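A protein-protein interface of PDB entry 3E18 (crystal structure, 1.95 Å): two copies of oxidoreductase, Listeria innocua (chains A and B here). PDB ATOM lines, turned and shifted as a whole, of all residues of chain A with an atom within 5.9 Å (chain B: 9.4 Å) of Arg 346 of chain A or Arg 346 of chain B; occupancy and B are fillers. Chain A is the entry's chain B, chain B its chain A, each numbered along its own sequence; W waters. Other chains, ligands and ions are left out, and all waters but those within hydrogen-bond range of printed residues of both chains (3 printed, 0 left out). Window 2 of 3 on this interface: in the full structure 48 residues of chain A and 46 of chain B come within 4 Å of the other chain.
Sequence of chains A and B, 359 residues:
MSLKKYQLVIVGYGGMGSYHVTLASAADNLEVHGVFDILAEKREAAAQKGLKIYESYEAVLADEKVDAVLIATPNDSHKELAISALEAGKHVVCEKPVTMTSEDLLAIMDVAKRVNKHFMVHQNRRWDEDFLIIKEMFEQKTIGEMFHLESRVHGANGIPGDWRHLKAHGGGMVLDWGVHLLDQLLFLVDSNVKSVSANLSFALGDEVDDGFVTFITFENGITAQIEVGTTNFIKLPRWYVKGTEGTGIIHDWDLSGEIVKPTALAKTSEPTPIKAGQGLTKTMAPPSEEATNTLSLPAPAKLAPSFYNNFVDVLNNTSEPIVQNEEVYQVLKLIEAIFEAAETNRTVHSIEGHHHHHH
The side-chain hydroxyl (OG) of Ser 195 of chain B is in hydrogen-bond range of the side-chain amide nitrogen (ND2) of Asn 345 of chain A, at 3.2 Å. A ring nitrogen (NE2) of His 349 of chain A is in hydrogen-bond range of the backbone carbonyl oxygen (O) of Asn 345 of chain B (2.7 Å). OG1 of Thr 347 of chain B lies within hydrogen-bond range of OG1 of Thr 347 of chain A (2.9 Å). O of Asn 345 of chain A sits at hydrogen-bond distance from NE2 of His 349 of chain B (2.8 Å). NH2 of Arg 346 of chain A lies close to NH1 of Arg 346 of chain B (3.3 Å).
N of Thr 217 of chain B is in hydrogen-bond range of O of Ser 195 of chain B (3.0 Å). The backbone carbonyl oxygen of Ala 341 of chain B lies within hydrogen-bond range of the backbone NH of Arg 346 of chain B. O of Thr 347 of chain B lies close to ND1 of His 349 of chain B. The backbone carbonyl oxygen (O) of Ala 341 of chain A lies within hydrogen-bond range of the backbone NH (N) of Arg 346 of chain A. The backbone carbonyl oxygen (O) of Thr 347 of chain A lies close to a ring nitrogen (ND1) of His 349 of chain A (3.4 Å).
Asn 345 of chain A touches Thr 347 of chain B. Arg 346 of chain A touches Thr 347 of chain B. Thr 347 of chain A touches Asn 345 of chain B. Arg 346 of chain B touches Thr 347 of chain A. His 349 of chain A touches Arg 346 of chain B.
Of the printed residues of chain B, Arg 346 of chain A touches Arg 346 and Thr 347. Of chain A, only Arg 346 (3.3 Å), Thr 347 (3.7 Å) and His 349 (3.95 Å) come within 4 Å of Arg 346 of chain B. Ala 341 of chain A touches none of the printed residues of chain B. No residue of chain B comes within 4 Å of Thr 344 of chain A. Of chain B, only Asn 345 (3.5 Å), Arg 346 (3.7 Å) and Thr 347 (2.9 Å) come within 4 Å of Thr 347 of chain A. Printed residues of chain B within 4 Å of His 349 of chain A: Asn 345 (2.7 Å) and Arg 346 (3.95 Å). Of the printed residues of chain B, Asn 345 of chain A touches Ser 195, Thr 347 and His 349. Of the printed residues of chain A, Ser 195 of chain B touches Asn 345. Of the printed residues of chain A, His 349 of chain B touches Asn 345. Glu 340 of chain A touches none of the printed residues of chain B. Ala 341 of chain B touches none of the printed residues of chain A. The nearest residue of chain B that does not touch Arg 346 of chain A is His 349 of chain B (4.3 Å). The nearest printed residue of chain B that does not touch Asn 345 of chain A is Thr 217 of chain B (4.8 Å).
Hydrophobic or aromatic side chains of chain A that line the printed part of chain B: His 349. Of the 22 printed residues of chain B, 5 touch a printed residue of chain A. Hydrophobic or aromatic side chains of chain B that line the printed part of chain A: His 349. Along chain B the printed residues that touch a printed residue of chain A span positions 195 to 349. Among the printed residues, no Asp or Glu carboxylate lies within 4 Å of a Lys or Arg side-chain nitrogen of the other chain.
Asn 345 of chain A touches His 349 of chain B, and with the chains exchanged His 349 of chain A touches Asn 345 of chain B. Arg 346 of chain A touches its own counterpart, Arg 346 of chain B. Arg 346 of chain A touches Thr 347 of chain B, and with the chains exchanged Thr 347 of chain A touches Arg 346 of chain B. His 349 of chain A touches Arg 346 of chain B, but with the chains exchanged Arg 346 of chain A does not touch His 349 of chain B (4.3 Å). Positions printed for both chains: 196, 197, 198, 340, 341, 342, 344, 345, 346, 347, 348 and 349.
Water W3 lies within hydrogen-bond range of NH1 of Arg 346 of chain A (2.4 Å), O of Thr 347 of chain A (2.7 Å) and NH1 of Arg 346 of chain B (3.2 Å). Water W2 lies within hydrogen-bond range of OG of Ser 197 of chain B and OG of Ser 197 of chain A. Water W1 bridges OG of Ser 197 of chain A (3.0 Å) and OG of Ser 197 of chain B (3.1 Å).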
ATOM      1  N   VAL A 196       0.494 -30.551  19.436  1.00  0.00           N
ATOM      2  CA  VAL A 196      -0.903 -30.766  19.769  1.00  0.00           C
ATOM      3  C   VAL A 196      -1.095 -30.507  21.253  1.00  0.00           C
ATOM      4  O   VAL A 196      -0.394 -31.094  22.060  1.00  0.00           O
ATOM      5  CB  VAL A 196      -1.332 -32.256  19.531  1.00  0.00           C
ATOM      6  CG1 VAL A 196      -2.814 -32.456  19.885  1.00  0.00           C
ATOM      7  CG2 VAL A 196      -1.068 -32.704  18.106  1.00  0.00           C
ATOM      8  N   SER A 197      -2.021 -29.630  21.627  1.00  0.00           N
ATOM      9  CA  SER A 197      -2.480 -29.611  23.022  1.00  0.00           C
ATOM     10  C   SER A 197      -3.977 -29.824  23.057  1.00  0.00           C
ATOM     11  O   SER A 197      -4.685 -29.441  22.125  1.00  0.00           O
ATOM     12  CB  SER A 197      -2.084 -28.323  23.764  1.00  0.00           C
ATOM     13  OG  SER A 197      -2.847 -27.201  23.340  1.00  0.00           O
ATOM     14  N   ALA A 198      -4.481 -30.441  24.121  1.00  0.00           N
ATOM     15  CA  ALA A 198      -5.911 -30.678  24.170  1.00  0.00           C
ATOM     16  C   ALA A 198      -6.498 -30.751  25.560  1.00  0.00           C
ATOM     17  O   ALA A 198      -5.803 -31.078  26.525  1.00  0.00           O
ATOM     18  CB  ALA A 198      -6.285 -31.962  23.372  1.00  0.00           C
ATOM     19  N   GLU A 340      -3.536 -38.386  24.453  1.00  0.00           N
ATOM     20  CA  GLU A 340      -2.320 -38.383  25.284  1.00  0.00           C
ATOM     21  C   GLU A 340      -2.071 -37.000  25.903  1.00  0.00           C
ATOM     22  O   GLU A 340      -1.791 -36.878  27.098  1.00  0.00           O
ATOM     23  CB  GLU A 340      -1.119 -38.858  24.445  1.00  0.00           C
ATOM     24  CG  GLU A 340       0.266 -38.631  25.064  1.00  0.00           C
ATOM     25  CD  GLU A 340       0.607 -39.597  26.193  1.00  0.00           C
ATOM     26  OE1 GLU A 340      -0.215 -40.479  26.535  1.00  0.00           O
ATOM     27  OE2 GLU A 340       1.723 -39.472  26.744  1.00  0.00           O
ATOM     28  N   ALA A 341      -2.221 -35.969  25.072  1.00  0.00           N
ATOM     29  CA  ALA A 341      -2.118 -34.564  25.467  1.00  0.00           C
ATOM     30  C   ALA A 341      -3.128 -34.122  26.527  1.00  0.00           C
ATOM     31  O   ALA A 341      -2.781 -33.373  27.444  1.00  0.00           O
ATOM     32  CB  ALA A 341      -2.258 -33.683  24.235  1.00  0.00           C
ATOM     33  N   ALA A 342      -4.384 -34.544  26.382  1.00  0.00           N
ATOM     34  CA  ALA A 342      -5.422 -34.210  27.344  1.00  0.00           C
ATOM     35  C   ALA A 342      -5.180 -34.940  28.668  1.00  0.00           C
ATOM     36  O   ALA A 342      -5.252 -34.330  29.717  1.00  0.00           O
ATOM     37  CB  ALA A 342      -6.791 -34.589  26.796  1.00  0.00           C
ATOM     38  N   THR A 344      -2.409 -36.367  30.021  1.00  0.00           N
ATOM     39  CA  THR A 344      -1.210 -35.927  30.736  1.00  0.00           C
ATOM     40  C   THR A 344      -1.154 -34.412  30.970  1.00  0.00           C
ATOM     41  O   THR A 344      -0.281 -33.936  31.700  1.00  0.00           O
ATOM     42  CB  THR A 344       0.077 -36.359  30.011  1.00  0.00           C
ATOM     43  OG1 THR A 344       0.106 -35.775  28.706  1.00  0.00           O
ATOM     44  CG2 THR A 344       0.163 -37.878  29.896  1.00  0.00           C
ATOM     45  N   ASN A 345      -2.072 -33.668  30.344  1.00  0.00           N
ATOM     46  CA  ASN A 345      -2.113 -32.205  30.423  1.00  0.00           C
ATOM     47  C   ASN A 345      -0.791 -31.577  29.951  1.00  0.00           C
ATOM     48  O   ASN A 345      -0.249 -30.667  30.579  1.00  0.00           O
ATOM     49  CB  ASN A 345      -2.539 -31.741  31.842  1.00  0.00           C
ATOM     50  CG  ASN A 345      -2.832 -30.250  31.928  1.00  0.00           C
ATOM     51  OD1 ASN A 345      -3.331 -29.623  30.988  1.00  0.00           O
ATOM     52  ND2 ASN A 345      -2.516 -29.674  33.076  1.00  0.00           N
ATOM     53  N   ARG A 346      -0.260 -32.103  28.847  1.00  0.00           N
ATOM     54  CA  ARG A 346       1.016 -31.641  28.279  1.00  0.00           C
ATOM     55  C   ARG A 346       0.820 -31.270  26.823  1.00  0.00           C
ATOM     56  O   ARG A 346      -0.173 -31.664  26.210  1.00  0.00           O
ATOM     57  CB  ARG A 346       2.098 -32.712  28.392  1.00  0.00           C
ATOM     58  CG  ARG A 346       2.451 -33.038  29.839  1.00  0.00           C
ATOM     59  CD  ARG A 346       3.611 -34.022  29.967  1.00  0.00           C
ATOM     60  NE  ARG A 346       4.878 -33.388  30.352  1.00  0.00           N
ATOM     61  CZ  ARG A 346       5.949 -33.308  29.561  1.00  0.00           C
ATOM     62  NH1 ARG A 346       5.906 -33.819  28.338  1.00  0.00           N
ATOM     63  NH2 ARG A 346       7.065 -32.726  29.992  1.00  0.00           N
ATOM     64  N   THR A 347       1.748 -30.494  26.283  1.00  0.00           N
ATOM     65  CA  THR A 347       1.801 -30.306  24.841  1.00  0.00           C
ATOM     66  C   THR A 347       2.694 -31.382  24.225  1.00  0.00           C
ATOM     67  O   THR A 347       3.815 -31.607  24.668  1.00  0.00           O
ATOM     68  CB  THR A 347       2.307 -28.920  24.465  1.00  0.00           C
ATOM     69  OG1 THR A 347       1.406 -27.940  24.991  1.00  0.00           O
ATOM     70  CG2 THR A 347       2.406 -28.772  22.941  1.00  0.00           C
ATOM     71  N   VAL A 348       2.157 -32.071  23.223  1.00  0.00           N
ATOM     72  CA  VAL A 348       2.864 -33.122  22.528  1.00  0.00           C
ATOM     73  C   VAL A 348       3.419 -32.559  21.203  1.00  0.00           C
ATOM     74  O   VAL A 348       2.817 -31.660  20.634  1.00  0.00           O
ATOM     75  CB  VAL A 348       1.897 -34.322  22.439  1.00  0.00           C
ATOM     76  CG1 VAL A 348       1.658 -34.783  21.056  1.00  0.00           C
ATOM     77  CG2 VAL A 348       2.331 -35.411  23.433  1.00  0.00           C
ATOM     78  N   HIS A 349       4.578 -33.047  20.738  1.00  0.00           N
ATOM     79  CA  HIS A 349       5.272 -32.406  19.612  1.00  0.00           C
ATOM     80  C   HIS A 349       5.452 -33.249  18.358  1.00  0.00           C
ATOM     81  O   HIS A 349       6.314 -32.944  17.510  1.00  0.00           O
ATOM     82  CB  HIS A 349       6.611 -31.804  20.057  1.00  0.00           C
ATOM     83  CG  HIS A 349       6.478 -30.907  21.240  1.00  0.00           C
ATOM     84  ND1 HIS A 349       6.475 -31.387  22.536  1.00  0.00           N
ATOM     85  CD2 HIS A 349       6.274 -29.574  21.326  1.00  0.00           C
ATOM     86  CE1 HIS A 349       6.313 -30.374  23.370  1.00  0.00           C
ATOM     87  NE2 HIS A 349       6.179 -29.266  22.661  1.00  0.00           N
ATOM     88  N   SER B 195      -2.511 -24.891  35.257  1.00  0.00           N
ATOM     89  CA  SER B 195      -1.727 -24.983  34.027  1.00  0.00           C
ATOM     90  C   SER B 195      -2.083 -23.909  33.010  1.00  0.00           C
ATOM     91  O   SER B 195      -3.178 -23.350  33.048  1.00  0.00           O
ATOM     92  CB  SER B 195      -1.893 -26.371  33.401  1.00  0.00           C
ATOM     93  OG  SER B 195      -3.219 -26.578  32.924  1.00  0.00           O
ATOM     94  N   VAL B 196      -1.145 -23.631  32.105  1.00  0.00           N
ATOM     95  CA  VAL B 196      -1.304 -22.604  31.055  1.00  0.00           C
ATOM     96  C   VAL B 196      -0.621 -23.094  29.787  1.00  0.00           C
ATOM     97  O   VAL B 196       0.542 -23.509  29.835  1.00  0.00           O
ATOM     98  CB  VAL B 196      -0.562 -21.282  31.424  1.00  0.00           C
ATOM     99  CG1 VAL B 196      -0.954 -20.151  30.480  1.00  0.00           C
ATOM    100  CG2 VAL B 196      -0.793 -20.890  32.850  1.00  0.00           C
ATOM    101  N   SER B 197      -1.311 -23.019  28.649  1.00  0.00           N
ATOM    102  CA  SER B 197      -0.652 -23.183  27.366  1.00  0.00           C
ATOM    103  C   SER B 197      -0.988 -21.890  26.635  1.00  0.00           C
ATOM    104  O   SER B 197      -1.983 -21.263  26.949  1.00  0.00           O
ATOM    105  CB  SER B 197      -1.220 -24.386  26.617  1.00  0.00           C
ATOM    106  OG  SER B 197      -2.585 -24.223  26.280  1.00  0.00           O
ATOM    107  N   ALA B 198      -0.152 -21.490  25.704  1.00  0.00           N
ATOM    108  CA  ALA B 198      -0.372 -20.220  24.987  1.00  0.00           C
ATOM    109  C   ALA B 198       0.332 -20.234  23.674  1.00  0.00           C
ATOM    110  O   ALA B 198       1.298 -20.972  23.475  1.00  0.00           O
ATOM    111  CB  ALA B 198       0.122 -19.016  25.827  1.00  0.00           C
ATOM    112  N   ASN B 199      -0.170 -19.409  22.766  1.00  0.00           N
ATOM    113  CA  ASN B 199       0.495 -19.182  21.497  1.00  0.00           C
ATOM    114  C   ASN B 199       0.319 -17.715  21.193  1.00  0.00           C
ATOM    115  O   ASN B 199      -0.721 -17.132  21.480  1.00  0.00           O
ATOM    116  CB  ASN B 199      -0.049 -20.128  20.391  1.00  0.00           C
ATOM    117  CG  ASN B 199      -0.343 -19.391  19.076  1.00  0.00           C
ATOM    118  OD1 ASN B 199       0.573 -19.040  18.303  1.00  0.00           O
ATOM    119  ND2 ASN B 199      -1.634 -19.191  18.797  1.00  0.00           N
ATOM    120  N   VAL B 213      -3.477 -16.290  22.387  1.00  0.00           N
ATOM    121  CA  VAL B 213      -4.553 -17.058  22.951  1.00  0.00           C
ATOM    122  C   VAL B 213      -3.897 -17.880  24.049  1.00  0.00           C
ATOM    123  O   VAL B 213      -2.743 -18.265  23.920  1.00  0.00           O
ATOM    124  CB  VAL B 213      -5.276 -17.942  21.883  1.00  0.00           C
ATOM    125  CG1 VAL B 213      -4.276 -18.684  21.001  1.00  0.00           C
ATOM    126  CG2 VAL B 213      -6.264 -18.908  22.534  1.00  0.00           C
ATOM    127  N   THR B 214      -4.613 -18.095  25.136  1.00  0.00           N
ATOM    128  CA  THR B 214      -4.131 -18.945  26.203  1.00  0.00           C
ATOM    129  C   THR B 214      -5.255 -19.829  26.738  1.00  0.00           C
ATOM    130  O   THR B 214      -6.401 -19.415  26.765  1.00  0.00           O
ATOM    131  CB  THR B 214      -3.444 -18.102  27.318  1.00  0.00           C
ATOM    132  OG1 THR B 214      -3.072 -18.950  28.410  1.00  0.00           O
ATOM    133  CG2 THR B 214      -4.350 -16.991  27.823  1.00  0.00           C
ATOM    134  N   PHE B 215      -4.933 -21.054  27.163  1.00  0.00           N
ATOM    135  CA  PHE B 215      -5.939 -21.912  27.743  1.00  0.00           C
ATOM    136  C   PHE B 215      -5.450 -22.196  29.145  1.00  0.00           C
ATOM    137  O   PHE B 215      -4.348 -22.727  29.335  1.00  0.00           O
ATOM    138  CB  PHE B 215      -6.105 -23.219  26.942  1.00  0.00           C
ATOM    139  CG  PHE B 215      -7.374 -24.000  27.278  1.00  0.00           C
ATOM    140  CD1 PHE B 215      -8.540 -23.797  26.554  1.00  0.00           C
ATOM    141  CD2 PHE B 215      -7.391 -24.946  28.313  1.00  0.00           C
ATOM    142  CE1 PHE B 215      -9.716 -24.508  26.848  1.00  0.00           C
ATOM    143  CE2 PHE B 215      -8.549 -25.654  28.611  1.00  0.00           C
ATOM    144  CZ  PHE B 215      -9.720 -25.438  27.869  1.00  0.00           C
ATOM    145  N   THR B 217      -6.157 -23.680  33.087  1.00  0.00           N
ATOM    146  CA  THR B 217      -6.926 -24.575  33.932  1.00  0.00           C
ATOM    147  C   THR B 217      -6.632 -24.234  35.401  1.00  0.00           C
ATOM    148  O   THR B 217      -5.476 -23.982  35.759  1.00  0.00           O
ATOM    149  CB  THR B 217      -6.572 -26.059  33.659  1.00  0.00           C
ATOM    150  OG1 THR B 217      -6.610 -26.310  32.250  1.00  0.00           O
ATOM    151  CG2 THR B 217      -7.559 -26.982  34.335  1.00  0.00           C
ATOM    152  N   ALA B 337       4.161 -17.105  32.957  1.00  0.00           N
ATOM    153  CA  ALA B 337       3.797 -18.461  32.498  1.00  0.00           C
ATOM    154  C   ALA B 337       3.357 -18.485  31.035  1.00  0.00           C
ATOM    155  O   ALA B 337       3.709 -19.398  30.296  1.00  0.00           O
ATOM    156  CB  ALA B 337       2.723 -19.065  33.375  1.00  0.00           C
ATOM    157  N   ILE B 338       2.608 -17.469  30.620  1.00  0.00           N
ATOM    158  CA  ILE B 338       2.108 -17.398  29.245  1.00  0.00           C
ATOM    159  C   ILE B 338       3.278 -17.252  28.285  1.00  0.00           C
ATOM    160  O   ILE B 338       3.351 -17.963  27.278  1.00  0.00           O
ATOM    161  CB  ILE B 338       1.086 -16.244  29.089  1.00  0.00           C
ATOM    162  CG1 ILE B 338      -0.271 -16.697  29.634  1.00  0.00           C
ATOM    163  CG2 ILE B 338       0.956 -15.780  27.637  1.00  0.00           C
ATOM    164  CD1 ILE B 338      -1.267 -15.566  29.842  1.00  0.00           C
ATOM    165  N   PHE B 339       4.194 -16.340  28.602  1.00  0.00           N
ATOM    166  CA  PHE B 339       5.349 -16.090  27.739  1.00  0.00           C
ATOM    167  C   PHE B 339       6.254 -17.307  27.627  1.00  0.00           C
ATOM    168  O   PHE B 339       6.732 -17.646  26.539  1.00  0.00           O
ATOM    169  CB  PHE B 339       6.123 -14.885  28.240  1.00  0.00           C
ATOM    170  CG  PHE B 339       5.547 -13.586  27.779  1.00  0.00           C
ATOM    171  CD1 PHE B 339       5.279 -13.382  26.426  1.00  0.00           C
ATOM    172  CD2 PHE B 339       5.278 -12.568  28.678  1.00  0.00           C
ATOM    173  CE1 PHE B 339       4.747 -12.188  25.985  1.00  0.00           C
ATOM    174  CE2 PHE B 339       4.754 -11.348  28.230  1.00  0.00           C
ATOM    175  CZ  PHE B 339       4.493 -11.167  26.890  1.00  0.00           C
ATOM    176  N   GLU B 340       6.457 -17.971  28.759  1.00  0.00           N
ATOM    177  CA  GLU B 340       7.217 -19.206  28.809  1.00  0.00           C
ATOM    178  C   GLU B 340       6.538 -20.322  27.999  1.00  0.00           C
ATOM    179  O   GLU B 340       7.206 -21.035  27.235  1.00  0.00           O
ATOM    180  CB  GLU B 340       7.403 -19.640  30.263  1.00  0.00           C
ATOM    181  CG  GLU B 340       8.297 -20.875  30.412  1.00  0.00           C
ATOM    182  CD  GLU B 340       8.241 -21.498  31.792  1.00  0.00           C
ATOM    183  OE1 GLU B 340       7.876 -20.805  32.773  1.00  0.00           O
ATOM    184  OE2 GLU B 340       8.571 -22.698  31.899  1.00  0.00           O
ATOM    185  N   ALA B 341       5.220 -20.464  28.158  1.00  0.00           N
ATOM    186  CA  ALA B 341       4.448 -21.491  27.447  1.00  0.00           C
ATOM    187  C   ALA B 341       4.550 -21.315  25.945  1.00  0.00           C
ATOM    188  O   ALA B 341       4.777 -22.277  25.212  1.00  0.00           O
ATOM    189  CB  ALA B 341       2.968 -21.477  27.901  1.00  0.00           C
ATOM    190  N   ALA B 342       4.415 -20.079  25.483  1.00  0.00           N
ATOM    191  CA  ALA B 342       4.521 -19.807  24.056  1.00  0.00           C
ATOM    192  C   ALA B 342       5.943 -19.941  23.481  1.00  0.00           C
ATOM    193  O   ALA B 342       6.123 -20.439  22.368  1.00  0.00           O
ATOM    194  CB  ALA B 342       3.960 -18.450  23.765  1.00  0.00           C
ATOM    195  N   GLU B 343       6.950 -19.494  24.226  1.00  0.00           N
ATOM    196  CA  GLU B 343       8.331 -19.591  23.737  1.00  0.00           C
ATOM    197  C   GLU B 343       8.870 -21.032  23.740  1.00  0.00           C
ATOM    198  O   GLU B 343       9.654 -21.389  22.874  1.00  0.00           O
ATOM    199  CB  GLU B 343       9.272 -18.610  24.469  1.00  0.00           C
ATOM    200  CG  GLU B 343       9.865 -19.104  25.784  1.00  0.00           C
ATOM    201  CD  GLU B 343      11.323 -18.694  25.975  1.00  0.00           C
ATOM    202  OE1 GLU B 343      12.009 -18.402  24.968  1.00  0.00           O
ATOM    203  OE2 GLU B 343      11.787 -18.680  27.138  1.00  0.00           O
ATOM    204  N   THR B 344       8.428 -21.863  24.680  1.00  0.00           N
ATOM    205  CA  THR B 344       8.880 -23.242  24.714  1.00  0.00           C
ATOM    206  C   THR B 344       7.896 -24.219  24.055  1.00  0.00           C
ATOM    207  O   THR B 344       8.183 -25.418  23.983  1.00  0.00           O
ATOM    208  CB  THR B 344       9.170 -23.709  26.151  1.00  0.00           C
ATOM    209  OG1 THR B 344       7.959 -23.704  26.912  1.00  0.00           O
ATOM    210  CG2 THR B 344      10.199 -22.784  26.820  1.00  0.00           C
ATOM    211  N   ASN B 345       6.762 -23.705  23.572  1.00  0.00           N
ATOM    212  CA  ASN B 345       5.655 -24.528  23.009  1.00  0.00           C
ATOM    213  C   ASN B 345       5.303 -25.704  23.921  1.00  0.00           C
ATOM    214  O   ASN B 345       5.245 -26.856  23.502  1.00  0.00           O
ATOM    215  CB  ASN B 345       5.988 -24.990  21.583  1.00  0.00           C
ATOM    216  CG  ASN B 345       4.778 -25.524  20.818  1.00  0.00           C
ATOM    217  OD1 ASN B 345       3.612 -25.301  21.180  1.00  0.00           O
ATOM    218  ND2 ASN B 345       5.061 -26.234  19.744  1.00  0.00           N
ATOM    219  N   ARG B 346       5.122 -25.393  25.197  1.00  0.00           N
ATOM    220  CA  ARG B 346       4.799 -26.386  26.188  1.00  0.00           C
ATOM    221  C   ARG B 346       3.661 -25.874  27.054  1.00  0.00           C
ATOM    222  O   ARG B 346       3.265 -24.710  26.947  1.00  0.00           O
ATOM    223  CB  ARG B 346       6.018 -26.673  27.051  1.00  0.00           C
ATOM    224  CG  ARG B 346       7.059 -27.581  26.389  1.00  0.00           C
ATOM    225  CD  ARG B 346       7.917 -28.248  27.457  1.00  0.00           C
ATOM    226  NE  ARG B 346       8.818 -29.270  26.919  1.00  0.00           N
ATOM    227  CZ  ARG B 346       8.512 -30.561  26.793  1.00  0.00           C
ATOM    228  NH1 ARG B 346       7.310 -31.011  27.139  1.00  0.00           N
ATOM    229  NH2 ARG B 346       9.414 -31.409  26.314  1.00  0.00           N
ATOM    230  N   THR B 347       3.117 -26.768  27.871  1.00  0.00           N
ATOM    231  CA  THR B 347       2.105 -26.416  28.849  1.00  0.00           C
ATOM    232  C   THR B 347       2.816 -26.265  30.190  1.00  0.00           C
ATOM    233  O   THR B 347       3.450 -27.199  30.684  1.00  0.00           O
ATOM    234  CB  THR B 347       0.989 -27.481  28.952  1.00  0.00           C
ATOM    235  OG1 THR B 347       0.409 -27.685  27.664  1.00  0.00           O
ATOM    236  CG2 THR B 347      -0.110 -27.016  29.918  1.00  0.00           C
ATOM    237  N   VAL B 348       2.694 -25.080  30.766  1.00  0.00           N
ATOM    238  CA  VAL B 348       3.406 -24.716  31.984  1.00  0.00           C
ATOM    239  C   VAL B 348       2.538 -25.068  33.180  1.00  0.00           C
ATOM    240  O   VAL B 348       1.391 -24.670  33.235  1.00  0.00           O
ATOM    241  CB  VAL B 348       3.747 -23.205  31.946  1.00  0.00           C
ATOM    242  CG1 VAL B 348       4.153 -22.667  33.317  1.00  0.00           C
ATOM    243  CG2 VAL B 348       4.847 -22.958  30.933  1.00  0.00           C
ATOM    244  N   HIS B 349       3.082 -25.828  34.127  1.00  0.00           N
ATOM    245  CA  HIS B 349       2.352 -26.199  35.338  1.00  0.00           C
ATOM    246  C   HIS B 349       2.795 -25.406  36.572  1.00  0.00           C
ATOM    247  O   HIS B 349       3.986 -25.152  36.750  1.00  0.00           O
ATOM    248  CB  HIS B 349       2.476 -27.701  35.573  1.00  0.00           C
ATOM    249  CG  HIS B 349       2.043 -28.515  34.398  1.00  0.00           C
ATOM    250  ND1 HIS B 349       2.922 -28.959  33.434  1.00  0.00           N
ATOM    251  CD2 HIS B 349       0.815 -28.929  34.008  1.00  0.00           C
ATOM    252  CE1 HIS B 349       2.255 -29.628  32.510  1.00  0.00           C
ATOM    253  NE2 HIS B 349       0.977 -29.629  32.838  1.00  0.00           N
HETATM  254  O   HOH W   1      -1.722 -24.446  23.297  1.00  0.00           O
HETATM  255  O   HOH W   2      -4.041 -26.398  25.642  1.00  0.00           O
HETATM  256  O   HOH W   3       5.441 -33.295  26.005  1.00  0.00           O
